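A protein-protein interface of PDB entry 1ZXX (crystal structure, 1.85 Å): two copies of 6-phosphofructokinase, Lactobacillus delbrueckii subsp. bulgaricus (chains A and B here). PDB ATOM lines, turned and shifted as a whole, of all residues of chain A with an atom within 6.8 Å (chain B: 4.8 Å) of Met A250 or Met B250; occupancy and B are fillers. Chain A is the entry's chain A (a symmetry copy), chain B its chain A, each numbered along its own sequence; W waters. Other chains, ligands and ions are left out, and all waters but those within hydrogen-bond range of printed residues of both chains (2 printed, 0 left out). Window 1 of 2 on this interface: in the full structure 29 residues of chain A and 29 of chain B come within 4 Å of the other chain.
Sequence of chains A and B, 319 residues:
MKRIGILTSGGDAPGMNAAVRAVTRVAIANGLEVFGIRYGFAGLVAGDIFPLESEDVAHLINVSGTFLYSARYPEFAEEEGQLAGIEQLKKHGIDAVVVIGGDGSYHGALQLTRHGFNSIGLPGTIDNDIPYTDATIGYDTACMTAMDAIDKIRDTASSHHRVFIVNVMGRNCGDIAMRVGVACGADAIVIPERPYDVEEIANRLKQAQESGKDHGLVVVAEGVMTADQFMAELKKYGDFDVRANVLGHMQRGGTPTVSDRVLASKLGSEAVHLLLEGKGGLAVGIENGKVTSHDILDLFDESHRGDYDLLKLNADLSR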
ATOM      1  N   PRO A  14     -10.584 -26.306  25.771  1.00  0.00           N
ATOM      2  CA  PRO A  14     -11.017 -27.695  25.539  1.00  0.00           C
ATOM      3  C   PRO A  14     -10.368 -28.622  26.571  1.00  0.00           C
ATOM      4  O   PRO A  14      -9.142 -28.586  26.758  1.00  0.00           O
ATOM      5  CB  PRO A  14     -10.504 -27.988  24.129  1.00  0.00           C
ATOM      6  CG  PRO A  14     -10.367 -26.611  23.467  1.00  0.00           C
ATOM      7  CD  PRO A  14      -9.854 -25.746  24.616  1.00  0.00           C
ATOM      8  N   THR A 141      -4.958 -28.877  22.128  1.00  0.00           N
ATOM      9  CA  THR A 141      -6.129 -28.754  21.238  1.00  0.00           C
ATOM     10  C   THR A 141      -6.023 -27.450  20.408  1.00  0.00           C
ATOM     11  O   THR A 141      -6.192 -27.446  19.185  1.00  0.00           O
ATOM     12  CB  THR A 141      -7.456 -28.830  22.029  1.00  0.00           C
ATOM     13  OG1 THR A 141      -7.534 -30.068  22.786  1.00  0.00           O
ATOM     14  CG2 THR A 141      -8.646 -28.918  21.066  1.00  0.00           C
ATOM     15  N   ALA A 142      -5.678 -26.357  21.082  1.00  0.00           N
ATOM     16  CA  ALA A 142      -5.478 -25.068  20.386  1.00  0.00           C
ATOM     17  C   ALA A 142      -4.404 -25.164  19.301  1.00  0.00           C
ATOM     18  O   ALA A 142      -4.569 -24.650  18.184  1.00  0.00           O
ATOM     19  CB  ALA A 142      -5.123 -23.970  21.408  1.00  0.00           C
ATOM     20  N   THR A 145      -5.910 -27.031  16.523  1.00  0.00           N
ATOM     21  CA  THR A 145      -6.869 -26.177  15.817  1.00  0.00           C
ATOM     22  C   THR A 145      -6.134 -25.233  14.885  1.00  0.00           C
ATOM     23  O   THR A 145      -6.492 -25.106  13.720  1.00  0.00           O
ATOM     24  CB  THR A 145      -7.722 -25.399  16.818  1.00  0.00           C
ATOM     25  OG1 THR A 145      -8.642 -26.304  17.445  1.00  0.00           O
ATOM     26  CG2 THR A 145      -8.644 -24.427  16.075  1.00  0.00           C
ATOM     27  N   ALA A 146      -5.101 -24.575  15.417  1.00  0.00           N
ATOM     28  CA  ALA A 146      -4.267 -23.670  14.638  1.00  0.00           C
ATOM     29  C   ALA A 146      -3.497 -24.382  13.534  1.00  0.00           C
ATOM     30  O   ALA A 146      -3.432 -23.893  12.413  1.00  0.00           O
ATOM     31  CB  ALA A 146      -3.309 -22.906  15.563  1.00  0.00           C
ATOM     32  N   ASP A 148      -4.336 -27.172  11.948  1.00  0.00           N
ATOM     33  CA  ASP A 148      -5.261 -27.611  10.887  1.00  0.00           C
ATOM     34  C   ASP A 148      -5.662 -26.401  10.048  1.00  0.00           C
ATOM     35  O   ASP A 148      -5.722 -26.480   8.819  1.00  0.00           O
ATOM     36  CB  ASP A 148      -6.524 -28.246  11.466  1.00  0.00           C
ATOM     37  CG  ASP A 148      -6.318 -29.699  11.906  1.00  0.00           C
ATOM     38  OD1 ASP A 148      -5.357 -30.358  11.472  1.00  0.00           O
ATOM     39  OD2 ASP A 148      -7.091 -30.223  12.706  1.00  0.00           O
ATOM     40  N   ALA A 149      -5.932 -25.284  10.714  1.00  0.00           N
ATOM     41  CA  ALA A 149      -6.286 -24.049   9.976  1.00  0.00           C
ATOM     42  C   ALA A 149      -5.137 -23.613   9.077  1.00  0.00           C
ATOM     43  O   ALA A 149      -5.342 -23.291   7.889  1.00  0.00           O
ATOM     44  CB  ALA A 149      -6.692 -22.946  10.944  1.00  0.00           C
ATOM     45  N   ILE A 150      -3.918 -23.617   9.610  1.00  0.00           N
ATOM     46  CA  ILE A 150      -2.757 -23.146   8.830  1.00  0.00           C
ATOM     47  C   ILE A 150      -2.319 -24.097   7.730  1.00  0.00           C
ATOM     48  O   ILE A 150      -1.774 -23.665   6.713  1.00  0.00           O
ATOM     49  CB  ILE A 150      -1.592 -22.750   9.743  1.00  0.00           C
ATOM     50  CG1 ILE A 150      -2.006 -21.552  10.597  1.00  0.00           C
ATOM     51  CG2 ILE A 150      -0.321 -22.433   8.922  1.00  0.00           C
ATOM     52  CD1 ILE A 150      -1.122 -21.325  11.842  1.00  0.00           C
ATOM     53  N   LYS A 152      -4.483 -25.516   5.865  1.00  0.00           N
ATOM     54  CA  LYS A 152      -5.413 -25.068   4.827  1.00  0.00           C
ATOM     55  C   LYS A 152      -4.883 -23.767   4.178  1.00  0.00           C
ATOM     56  O   LYS A 152      -4.890 -23.605   2.955  1.00  0.00           O
ATOM     57  CB  LYS A 152      -6.813 -24.872   5.415  1.00  0.00           C
ATOM     58  CG  LYS A 152      -7.493 -26.188   5.893  1.00  0.00           C
ATOM     59  CD  LYS A 152      -8.935 -25.983   6.333  1.00  0.00           C
ATOM     60  CE  LYS A 152      -9.542 -27.321   6.803  1.00  0.00           C
ATOM     61  NZ  LYS A 152      -8.780 -27.860   8.002  1.00  0.00           N
ATOM     62  N   ILE A 153      -4.392 -22.862   5.012  1.00  0.00           N
ATOM     63  CA  ILE A 153      -3.729 -21.671   4.500  1.00  0.00           C
ATOM     64  C   ILE A 153      -2.550 -22.047   3.591  1.00  0.00           C
ATOM     65  O   ILE A 153      -2.405 -21.471   2.528  1.00  0.00           O
ATOM     66  CB  ILE A 153      -3.315 -20.733   5.649  1.00  0.00           C
ATOM     67  CG1 ILE A 153      -4.555 -20.172   6.347  1.00  0.00           C
ATOM     68  CG2 ILE A 153      -2.444 -19.579   5.123  1.00  0.00           C
ATOM     69  CD1 ILE A 153      -4.230 -19.358   7.591  1.00  0.00           C
ATOM     70  N   THR A 156      -3.743 -23.054   0.032  1.00  0.00           N
ATOM     71  CA  THR A 156      -4.105 -21.951  -0.864  1.00  0.00           C
ATOM     72  C   THR A 156      -2.912 -21.055  -1.196  1.00  0.00           C
ATOM     73  O   THR A 156      -2.774 -20.594  -2.328  1.00  0.00           O
ATOM     74  CB  THR A 156      -5.361 -21.172  -0.348  1.00  0.00           C
ATOM     75  OG1 THR A 156      -5.692 -20.123  -1.281  1.00  0.00           O
ATOM     76  CG2 THR A 156      -5.098 -20.444   0.970  1.00  0.00           C
ATOM     77  N   PHE A 164       1.757 -15.804   3.567  1.00  0.00           N
ATOM     78  CA  PHE A 164       0.772 -15.484   4.573  1.00  0.00           C
ATOM     79  C   PHE A 164       1.409 -15.109   5.899  1.00  0.00           C
ATOM     80  O   PHE A 164       2.363 -15.753   6.358  1.00  0.00           O
ATOM     81  CB  PHE A 164      -0.227 -16.631   4.788  1.00  0.00           C
ATOM     82  CG  PHE A 164      -1.373 -16.629   3.820  1.00  0.00           C
ATOM     83  CD1 PHE A 164      -2.622 -16.138   4.208  1.00  0.00           C
ATOM     84  CD2 PHE A 164      -1.200 -17.106   2.518  1.00  0.00           C
ATOM     85  CE1 PHE A 164      -3.697 -16.140   3.325  1.00  0.00           C
ATOM     86  CE2 PHE A 164      -2.265 -17.107   1.611  1.00  0.00           C
ATOM     87  CZ  PHE A 164      -3.519 -16.630   2.016  1.00  0.00           C
ATOM     88  N   MET A 169      -3.262 -17.366  18.751  1.00  0.00           N
ATOM     89  CA  MET A 169      -3.487 -16.936  20.124  1.00  0.00           C
ATOM     90  C   MET A 169      -2.297 -17.234  21.036  1.00  0.00           C
ATOM     91  O   MET A 169      -1.252 -17.657  20.570  1.00  0.00           O
ATOM     92  CB  MET A 169      -4.800 -17.504  20.677  1.00  0.00           C
ATOM     93  CG  MET A 169      -5.991 -16.601  20.380  1.00  0.00           C
ATOM     94  SD  MET A 169      -7.602 -17.284  20.753  1.00  0.00           S
ATOM     95  CE  MET A 169      -8.657 -15.873  20.441  1.00  0.00           C
ATOM     96  N   ASN A 245      -3.994 -13.070   8.024  1.00  0.00           N
ATOM     97  CA  ASN A 245      -5.165 -13.659   8.653  1.00  0.00           C
ATOM     98  C   ASN A 245      -4.977 -13.668  10.153  1.00  0.00           C
ATOM     99  O   ASN A 245      -3.851 -13.786  10.641  1.00  0.00           O
ATOM    100  CB  ASN A 245      -5.387 -15.121   8.208  1.00  0.00           C
ATOM    101  CG  ASN A 245      -5.955 -15.264   6.795  1.00  0.00           C
ATOM    102  OD1 ASN A 245      -6.243 -16.391   6.376  1.00  0.00           O
ATOM    103  ND2 ASN A 245      -6.110 -14.152   6.047  1.00  0.00           N
ATOM    104  N   VAL A 246      -6.087 -13.584  10.872  1.00  0.00           N
ATOM    105  CA  VAL A 246      -6.116 -13.728  12.322  1.00  0.00           C
ATOM    106  C   VAL A 246      -7.030 -14.927  12.608  1.00  0.00           C
ATOM    107  O   VAL A 246      -8.225 -14.861  12.334  1.00  0.00           O
ATOM    108  CB  VAL A 246      -6.684 -12.450  13.022  1.00  0.00           C
ATOM    109  CG1 VAL A 246      -6.767 -12.647  14.532  1.00  0.00           C
ATOM    110  CG2 VAL A 246      -5.831 -11.229  12.679  1.00  0.00           C
ATOM    111  N   LEU A 247      -6.473 -16.021  13.128  1.00  0.00           N
ATOM    112  CA  LEU A 247      -7.287 -17.239  13.357  1.00  0.00           C
ATOM    113  C   LEU A 247      -8.466 -17.015  14.309  1.00  0.00           C
ATOM    114  O   LEU A 247      -9.571 -17.466  14.046  1.00  0.00           O
ATOM    115  CB  LEU A 247      -6.437 -18.451  13.810  1.00  0.00           C
ATOM    116  CG  LEU A 247      -5.314 -18.910  12.883  1.00  0.00           C
ATOM    117  CD1 LEU A 247      -4.663 -20.168  13.449  1.00  0.00           C
ATOM    118  CD2 LEU A 247      -5.792 -19.143  11.429  1.00  0.00           C
ATOM    119  N   GLY A 248      -8.258 -16.344  15.426  1.00  0.00           N
ATOM    120  CA  GLY A 248      -9.422 -16.018  16.253  1.00  0.00           C
ATOM    121  C   GLY A 248      -9.874 -17.108  17.217  1.00  0.00           C
ATOM    122  O   GLY A 248      -9.112 -18.035  17.516  1.00  0.00           O
ATOM    123  N   HIS A 249     -11.111 -16.983  17.693  1.00  0.00           N
ATOM    124  CA  HIS A 249     -11.569 -17.695  18.871  1.00  0.00           C
ATOM    125  C   HIS A 249     -11.854 -19.175  18.639  1.00  0.00           C
ATOM    126  O   HIS A 249     -12.132 -19.887  19.599  1.00  0.00           O
ATOM    127  CB  HIS A 249     -12.766 -17.006  19.511  1.00  0.00           C
ATOM    128  CG  HIS A 249     -12.406 -15.719  20.193  1.00  0.00           C
ATOM    129  ND1 HIS A 249     -12.130 -14.566  19.493  1.00  0.00           N
ATOM    130  CD2 HIS A 249     -12.226 -15.420  21.502  1.00  0.00           C
ATOM    131  CE1 HIS A 249     -11.830 -13.597  20.344  1.00  0.00           C
ATOM    132  NE2 HIS A 249     -11.871 -14.093  21.570  1.00  0.00           N
ATOM    133  N   MET A 250     -11.748 -19.619  17.389  1.00  0.00           N
ATOM    134  CA  MET A 250     -11.824 -21.069  17.083  1.00  0.00           C
ATOM    135  C   MET A 250     -10.761 -21.839  17.883  1.00  0.00           C
ATOM    136  O   MET A 250     -10.975 -23.007  18.270  1.00  0.00           O
ATOM    137  CB  MET A 250     -11.670 -21.324  15.585  1.00  0.00           C
ATOM    138  CG  MET A 250     -10.311 -20.942  14.995  1.00  0.00           C
ATOM    139  SD  MET A 250     -10.160 -21.174  13.223  1.00  0.00           S
ATOM    140  CE  MET A 250     -10.306 -22.959  13.101  1.00  0.00           C
ATOM    141  N   GLN A 251      -9.621 -21.180  18.127  1.00  0.00           N
ATOM    142  CA  GLN A 251      -8.532 -21.770  18.924  1.00  0.00           C
ATOM    143  C   GLN A 251      -8.934 -22.095  20.354  1.00  0.00           C
ATOM    144  O   GLN A 251      -8.244 -22.858  21.039  1.00  0.00           O
ATOM    145  CB  GLN A 251      -7.296 -20.863  18.933  1.00  0.00           C
ATOM    146  CG  GLN A 251      -6.622 -20.702  17.598  1.00  0.00           C
ATOM    147  CD  GLN A 251      -5.648 -19.535  17.583  1.00  0.00           C
ATOM    148  OE1 GLN A 251      -4.440 -19.733  17.702  1.00  0.00           O
ATOM    149  NE2 GLN A 251      -6.178 -18.312  17.461  1.00  0.00           N
ATOM    150  N   ARG A 252     -10.044 -21.536  20.813  1.00  0.00           N
ATOM    151  CA  ARG A 252     -10.502 -21.820  22.161  1.00  0.00           C
ATOM    152  C   ARG A 252     -11.472 -22.995  22.236  1.00  0.00           C
ATOM    153  O   ARG A 252     -11.843 -23.413  23.321  1.00  0.00           O
ATOM    154  CB  ARG A 252     -11.166 -20.589  22.761  1.00  0.00           C
ATOM    155  CG  ARG A 252     -10.154 -19.471  23.086  1.00  0.00           C
ATOM    156  CD  ARG A 252      -9.706 -19.500  24.538  1.00  0.00           C
ATOM    157  NE  ARG A 252     -10.850 -19.148  25.375  1.00  0.00           N
ATOM    158  CZ  ARG A 252     -11.271 -17.902  25.569  1.00  0.00           C
ATOM    159  NH1 ARG A 252     -12.341 -17.686  26.310  1.00  0.00           N
ATOM    160  NH2 ARG A 252     -10.615 -16.881  25.001  1.00  0.00           N
ATOM    161  N   GLY A 253     -11.909 -23.496  21.091  1.00  0.00           N
ATOM    162  CA  GLY A 253     -12.976 -24.497  21.098  1.00  0.00           C
ATOM    163  C   GLY A 253     -12.583 -25.770  20.379  1.00  0.00           C
ATOM    164  O   GLY A 253     -11.438 -25.943  19.976  1.00  0.00           O
ATOM    165  N   GLY A 254     -13.561 -26.657  20.211  1.00  0.00           N
ATOM    166  CA  GLY A 254     -13.336 -27.922  19.520  1.00  0.00           C
ATOM    167  C   GLY A 254     -13.215 -29.066  20.515  1.00  0.00           C
ATOM    168  O   GLY A 254     -12.867 -28.863  21.678  1.00  0.00           O
ATOM    169  N   THR B 145     -15.234 -26.318   6.174  1.00  0.00           N
ATOM    170  CA  THR B 145     -14.147 -25.626   6.871  1.00  0.00           C
ATOM    171  C   THR B 145     -14.715 -24.562   7.791  1.00  0.00           C
ATOM    172  O   THR B 145     -14.341 -24.484   8.955  1.00  0.00           O
ATOM    173  CB  THR B 145     -13.178 -25.010   5.862  1.00  0.00           C
ATOM    174  OG1 THR B 145     -12.420 -26.060   5.246  1.00  0.00           O
ATOM    175  CG2 THR B 145     -12.109 -24.195   6.595  1.00  0.00           C
ATOM    176  N   ALA B 149     -14.920 -24.533  11.962  1.00  0.00           N
ATOM    177  CA  ALA B 149     -14.367 -23.364  12.687  1.00  0.00           C
ATOM    178  C   ALA B 149     -15.427 -22.736  13.580  1.00  0.00           C
ATOM    179  O   ALA B 149     -15.171 -22.437  14.764  1.00  0.00           O
ATOM    180  CB  ALA B 149     -13.785 -22.354  11.707  1.00  0.00           C
ATOM    181  N   LYS B 152     -16.382 -24.467  16.813  1.00  0.00           N
ATOM    182  CA  LYS B 152     -15.391 -24.167  17.847  1.00  0.00           C
ATOM    183  C   LYS B 152     -15.699 -22.789  18.480  1.00  0.00           C
ATOM    184  O   LYS B 152     -15.664 -22.617  19.701  1.00  0.00           O
ATOM    185  CB  LYS B 152     -13.977 -24.212  17.258  1.00  0.00           C
ATOM    186  CG  LYS B 152     -13.524 -25.626  16.795  1.00  0.00           C
ATOM    187  CD  LYS B 152     -12.068 -25.666  16.354  1.00  0.00           C
ATOM    188  CE  LYS B 152     -11.690 -27.091  15.901  1.00  0.00           C
ATOM    189  NZ  LYS B 152     -12.532 -27.511  14.706  1.00  0.00           N
ATOM    190  N   ILE B 153     -16.035 -21.825  17.636  1.00  0.00           N
ATOM    191  CA  ILE B 153     -16.492 -20.536  18.133  1.00  0.00           C
ATOM    192  C   ILE B 153     -17.716 -20.703  19.046  1.00  0.00           C
ATOM    193  O   ILE B 153     -17.763 -20.099  20.102  1.00  0.00           O
ATOM    194  CB  ILE B 153     -16.748 -19.556  16.974  1.00  0.00           C
ATOM    195  CG1 ILE B 153     -15.434 -19.214  16.270  1.00  0.00           C
ATOM    196  CG2 ILE B 153     -17.416 -18.268  17.485  1.00  0.00           C
ATOM    197  CD1 ILE B 153     -15.621 -18.373  15.017  1.00  0.00           C
ATOM    198  N   ASN B 245     -14.820 -12.137  14.512  1.00  0.00           N
ATOM    199  CA  ASN B 245     -13.762 -12.917  13.891  1.00  0.00           C
ATOM    200  C   ASN B 245     -13.950 -12.913  12.391  1.00  0.00           C
ATOM    201  O   ASN B 245     -15.081 -12.848  11.904  1.00  0.00           O
ATOM    202  CB  ASN B 245     -13.783 -14.390  14.353  1.00  0.00           C
ATOM    203  CG  ASN B 245     -13.245 -14.610  15.768  1.00  0.00           C
ATOM    204  OD1 ASN B 245     -13.146 -15.764  16.200  1.00  0.00           O
ATOM    205  ND2 ASN B 245     -12.908 -13.529  16.503  1.00  0.00           N
ATOM    206  N   LEU B 247     -12.865 -15.513   9.444  1.00  0.00           N
ATOM    207  CA  LEU B 247     -12.262 -16.851   9.230  1.00  0.00           C
ATOM    208  C   LEU B 247     -11.063 -16.834   8.276  1.00  0.00           C
ATOM    209  O   LEU B 247     -10.047 -17.458   8.546  1.00  0.00           O
ATOM    210  CB  LEU B 247     -13.300 -17.912   8.790  1.00  0.00           C
ATOM    211  CG  LEU B 247     -14.483 -18.169   9.721  1.00  0.00           C
ATOM    212  CD1 LEU B 247     -15.333 -19.309   9.169  1.00  0.00           C
ATOM    213  CD2 LEU B 247     -14.048 -18.461  11.178  1.00  0.00           C
ATOM    214  N   GLY B 248     -11.160 -16.151   7.152  1.00  0.00           N
ATOM    215  CA  GLY B 248      -9.958 -16.031   6.322  1.00  0.00           C
ATOM    216  C   GLY B 248      -9.693 -17.191   5.371  1.00  0.00           C
ATOM    217  O   GLY B 248     -10.597 -17.984   5.082  1.00  0.00           O
ATOM    218  N   HIS B 249      -8.452 -17.277   4.895  1.00  0.00           N
ATOM    219  CA  HIS B 249      -8.119 -18.067   3.726  1.00  0.00           C
ATOM    220  C   HIS B 249      -8.080 -19.571   3.975  1.00  0.00           C
ATOM    221  O   HIS B 249      -7.925 -20.330   3.023  1.00  0.00           O
ATOM    222  CB  HIS B 249      -6.826 -17.592   3.079  1.00  0.00           C
ATOM    223  CG  HIS B 249      -6.970 -16.270   2.382  1.00  0.00           C
ATOM    224  ND1 HIS B 249      -7.051 -15.081   3.068  1.00  0.00           N
ATOM    225  CD2 HIS B 249      -7.099 -15.961   1.069  1.00  0.00           C
ATOM    226  CE1 HIS B 249      -7.189 -14.086   2.206  1.00  0.00           C
ATOM    227  NE2 HIS B 249      -7.231 -14.594   0.986  1.00  0.00           N
ATOM    228  N   MET B 250      -8.258 -19.978   5.230  1.00  0.00           N
ATOM    229  CA  MET B 250      -8.420 -21.417   5.552  1.00  0.00           C
ATOM    230  C   MET B 250      -9.596 -22.011   4.760  1.00  0.00           C
ATOM    231  O   MET B 250      -9.578 -23.202   4.386  1.00  0.00           O
ATOM    232  CB  MET B 250      -8.613 -21.626   7.052  1.00  0.00           C
ATOM    233  CG  MET B 250      -9.890 -21.019   7.637  1.00  0.00           C
ATOM    234  SD  MET B 250     -10.075 -21.203   9.411  1.00  0.00           S
ATOM    235  CE  MET B 250     -10.225 -22.986   9.554  1.00  0.00           C
ATOM    236  N   GLN B 251     -10.612 -21.176   4.507  1.00  0.00           N
ATOM    237  CA  GLN B 251     -11.784 -21.588   3.716  1.00  0.00           C
ATOM    238  C   GLN B 251     -11.444 -21.991   2.291  1.00  0.00           C
ATOM    239  O   GLN B 251     -12.249 -22.637   1.613  1.00  0.00           O
ATOM    240  CB  GLN B 251     -12.854 -20.489   3.695  1.00  0.00           C
ATOM    241  CG  GLN B 251     -13.492 -20.205   5.028  1.00  0.00           C
ATOM    242  CD  GLN B 251     -14.261 -18.894   5.029  1.00  0.00           C
ATOM    243  OE1 GLN B 251     -15.485 -18.892   4.911  1.00  0.00           O
ATOM    244  NE2 GLN B 251     -13.537 -17.773   5.137  1.00  0.00           N
ATOM    245  N   ARG B 252     -10.256 -21.627   1.826  1.00  0.00           N
ATOM    246  CA  ARG B 252      -9.853 -21.998   0.482  1.00  0.00           C
ATOM    247  C   ARG B 252      -9.089 -23.317   0.421  1.00  0.00           C
ATOM    248  O   ARG B 252      -8.794 -23.802  -0.659  1.00  0.00           O
ATOM    249  CB  ARG B 252      -8.996 -20.899  -0.132  1.00  0.00           C
ATOM    250  CG  ARG B 252      -9.810 -19.634  -0.471  1.00  0.00           C
ATOM    251  CD  ARG B 252     -10.258 -19.606  -1.923  1.00  0.00           C
ATOM    252  NE  ARG B 252      -9.073 -19.457  -2.762  1.00  0.00           N
ATOM    253  CZ  ARG B 252      -8.453 -18.298  -2.970  1.00  0.00           C
ATOM    254  NH1 ARG B 252      -7.362 -18.270  -3.713  1.00  0.00           N
ATOM    255  NH2 ARG B 252      -8.932 -17.177  -2.415  1.00  0.00           N
ATOM    256  N   GLY B 253      -8.740 -23.870   1.572  1.00  0.00           N
ATOM    257  CA  GLY B 253      -7.852 -25.033   1.577  1.00  0.00           C
ATOM    258  C   GLY B 253      -8.448 -26.216   2.310  1.00  0.00           C
ATOM    259  O   GLY B 253      -9.606 -26.193   2.714  1.00  0.00           O
HETATM  260  O   HOH W   1      -7.514 -18.543   7.579  1.00  0.00           O
HETATM  261  O   HOH W   2     -12.247 -18.108  15.023  1.00  0.00           O
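Water W1 lies within hydrogen-bond range of OD1 of Asn A245 (2.8 Å), N of Met B250 (2.9 Å), O of Leu B247 (2.9 Å) and N of His B249 (3.1 Å).
Water W2 lies within hydrogen-bond range of OD1 of Asn B245 (2.8 Å), N of Met A250 (2.9 Å), O of Leu A247 (2.9 Å) and N of His A249 (3.1 Å).
Lys A152 touches Met B250 (CB to O, 3.4 Å).
His B249 touches Thr A156.
Phe A164 touches His B249 (CE1 to CG, 3.4 Å).
Gly A248 touches Asn B245 (C to OD1, 3.7 Å).
CB of Met A250 touches O of Ala B149, at 3.8 Å.
Met A250 touches Lys B152.
Met A250 touches Ile B153 (N to CG1, 3.9 Å).
Met B250 touches Met A250.
Lys B152 touches Gly A253.
CG of Lys B152 touches CA of Gly A254 (3.6 Å).
Met A250 touches four residues of chain B.
Printed residues of chain A within 4 Å of Met B250: Ala A149 (3.8 Å), Lys A152 (3.4 Å), Ile A153 (3.9 Å) and Met A250 (3.5 Å).
Printed residues of chain A within 4 Å of Arg B252: Thr A156.
Printed residues of chain B within 4 Å of His A249: Asn B245 (2.8 Å).
Ala A146 touches none of the printed residues of chain B.
The nearest residue of chain B that does not touch Met A250 is Asn B245 (4.3 Å).
The nearest residue of chain A that does not touch Met B250 is Asn A245 (4.3 Å).
The nearest printed residue of chain B that does not touch Asn A245 is Met B250 (4.3 Å).
The backbone carbonyl oxygen of Gly B248 sits at hydrogen-bond distance from the side-chain amide nitrogen of Gln B251 (2.9 Å).
The side-chain amino group of Lys A152 lies close to the backbone carbonyl oxygen of Asp A148 (3.5 Å).
The backbone carbonyl oxygen (O) of Gly A248 is in hydrogen-bond range of the side-chain amide nitrogen (NE2) of Gln A251 (2.9 Å).
The side-chain hydroxyl (OG1) of Thr A145 sits at hydrogen-bond distance from the backbone carbonyl oxygen (O) of Thr A141 (3.2 Å).
Among the printed residues, 19 pairs touch across the chains.
Among the printed residues, no Asp or Glu carboxylate lies within 4 Å of a Lys or Arg side-chain nitrogen of the other chain.
Thr A145 touches Lys B152, and with the chains exchanged Lys A152 touches Thr B145.
Lys A152 touches Met B250, and with the chains exchanged Met A250 touches Lys B152.
Asn A245 touches Gly B248, and with the chains exchanged Gly A248 touches Asn B245.
Met A250 touches its own counterpart, Met B250.
12 positions are printed for both chains.
Of the 19 pairs that touch across the chains among the printed residues, 15 have their exchanged pair printed and touching as well.
The side-chain hydroxyl (OG1) of Thr A156 is in hydrogen-bond range of the guanidinium group (NH1) of Arg B252, 3.5 Å away.
The side-chain amide oxygen of Asn B245 lies within hydrogen-bond range of the backbone NH of His A249 (2.8 Å).
OD1 of Asn A245 lies within hydrogen-bond range of N of His B249.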
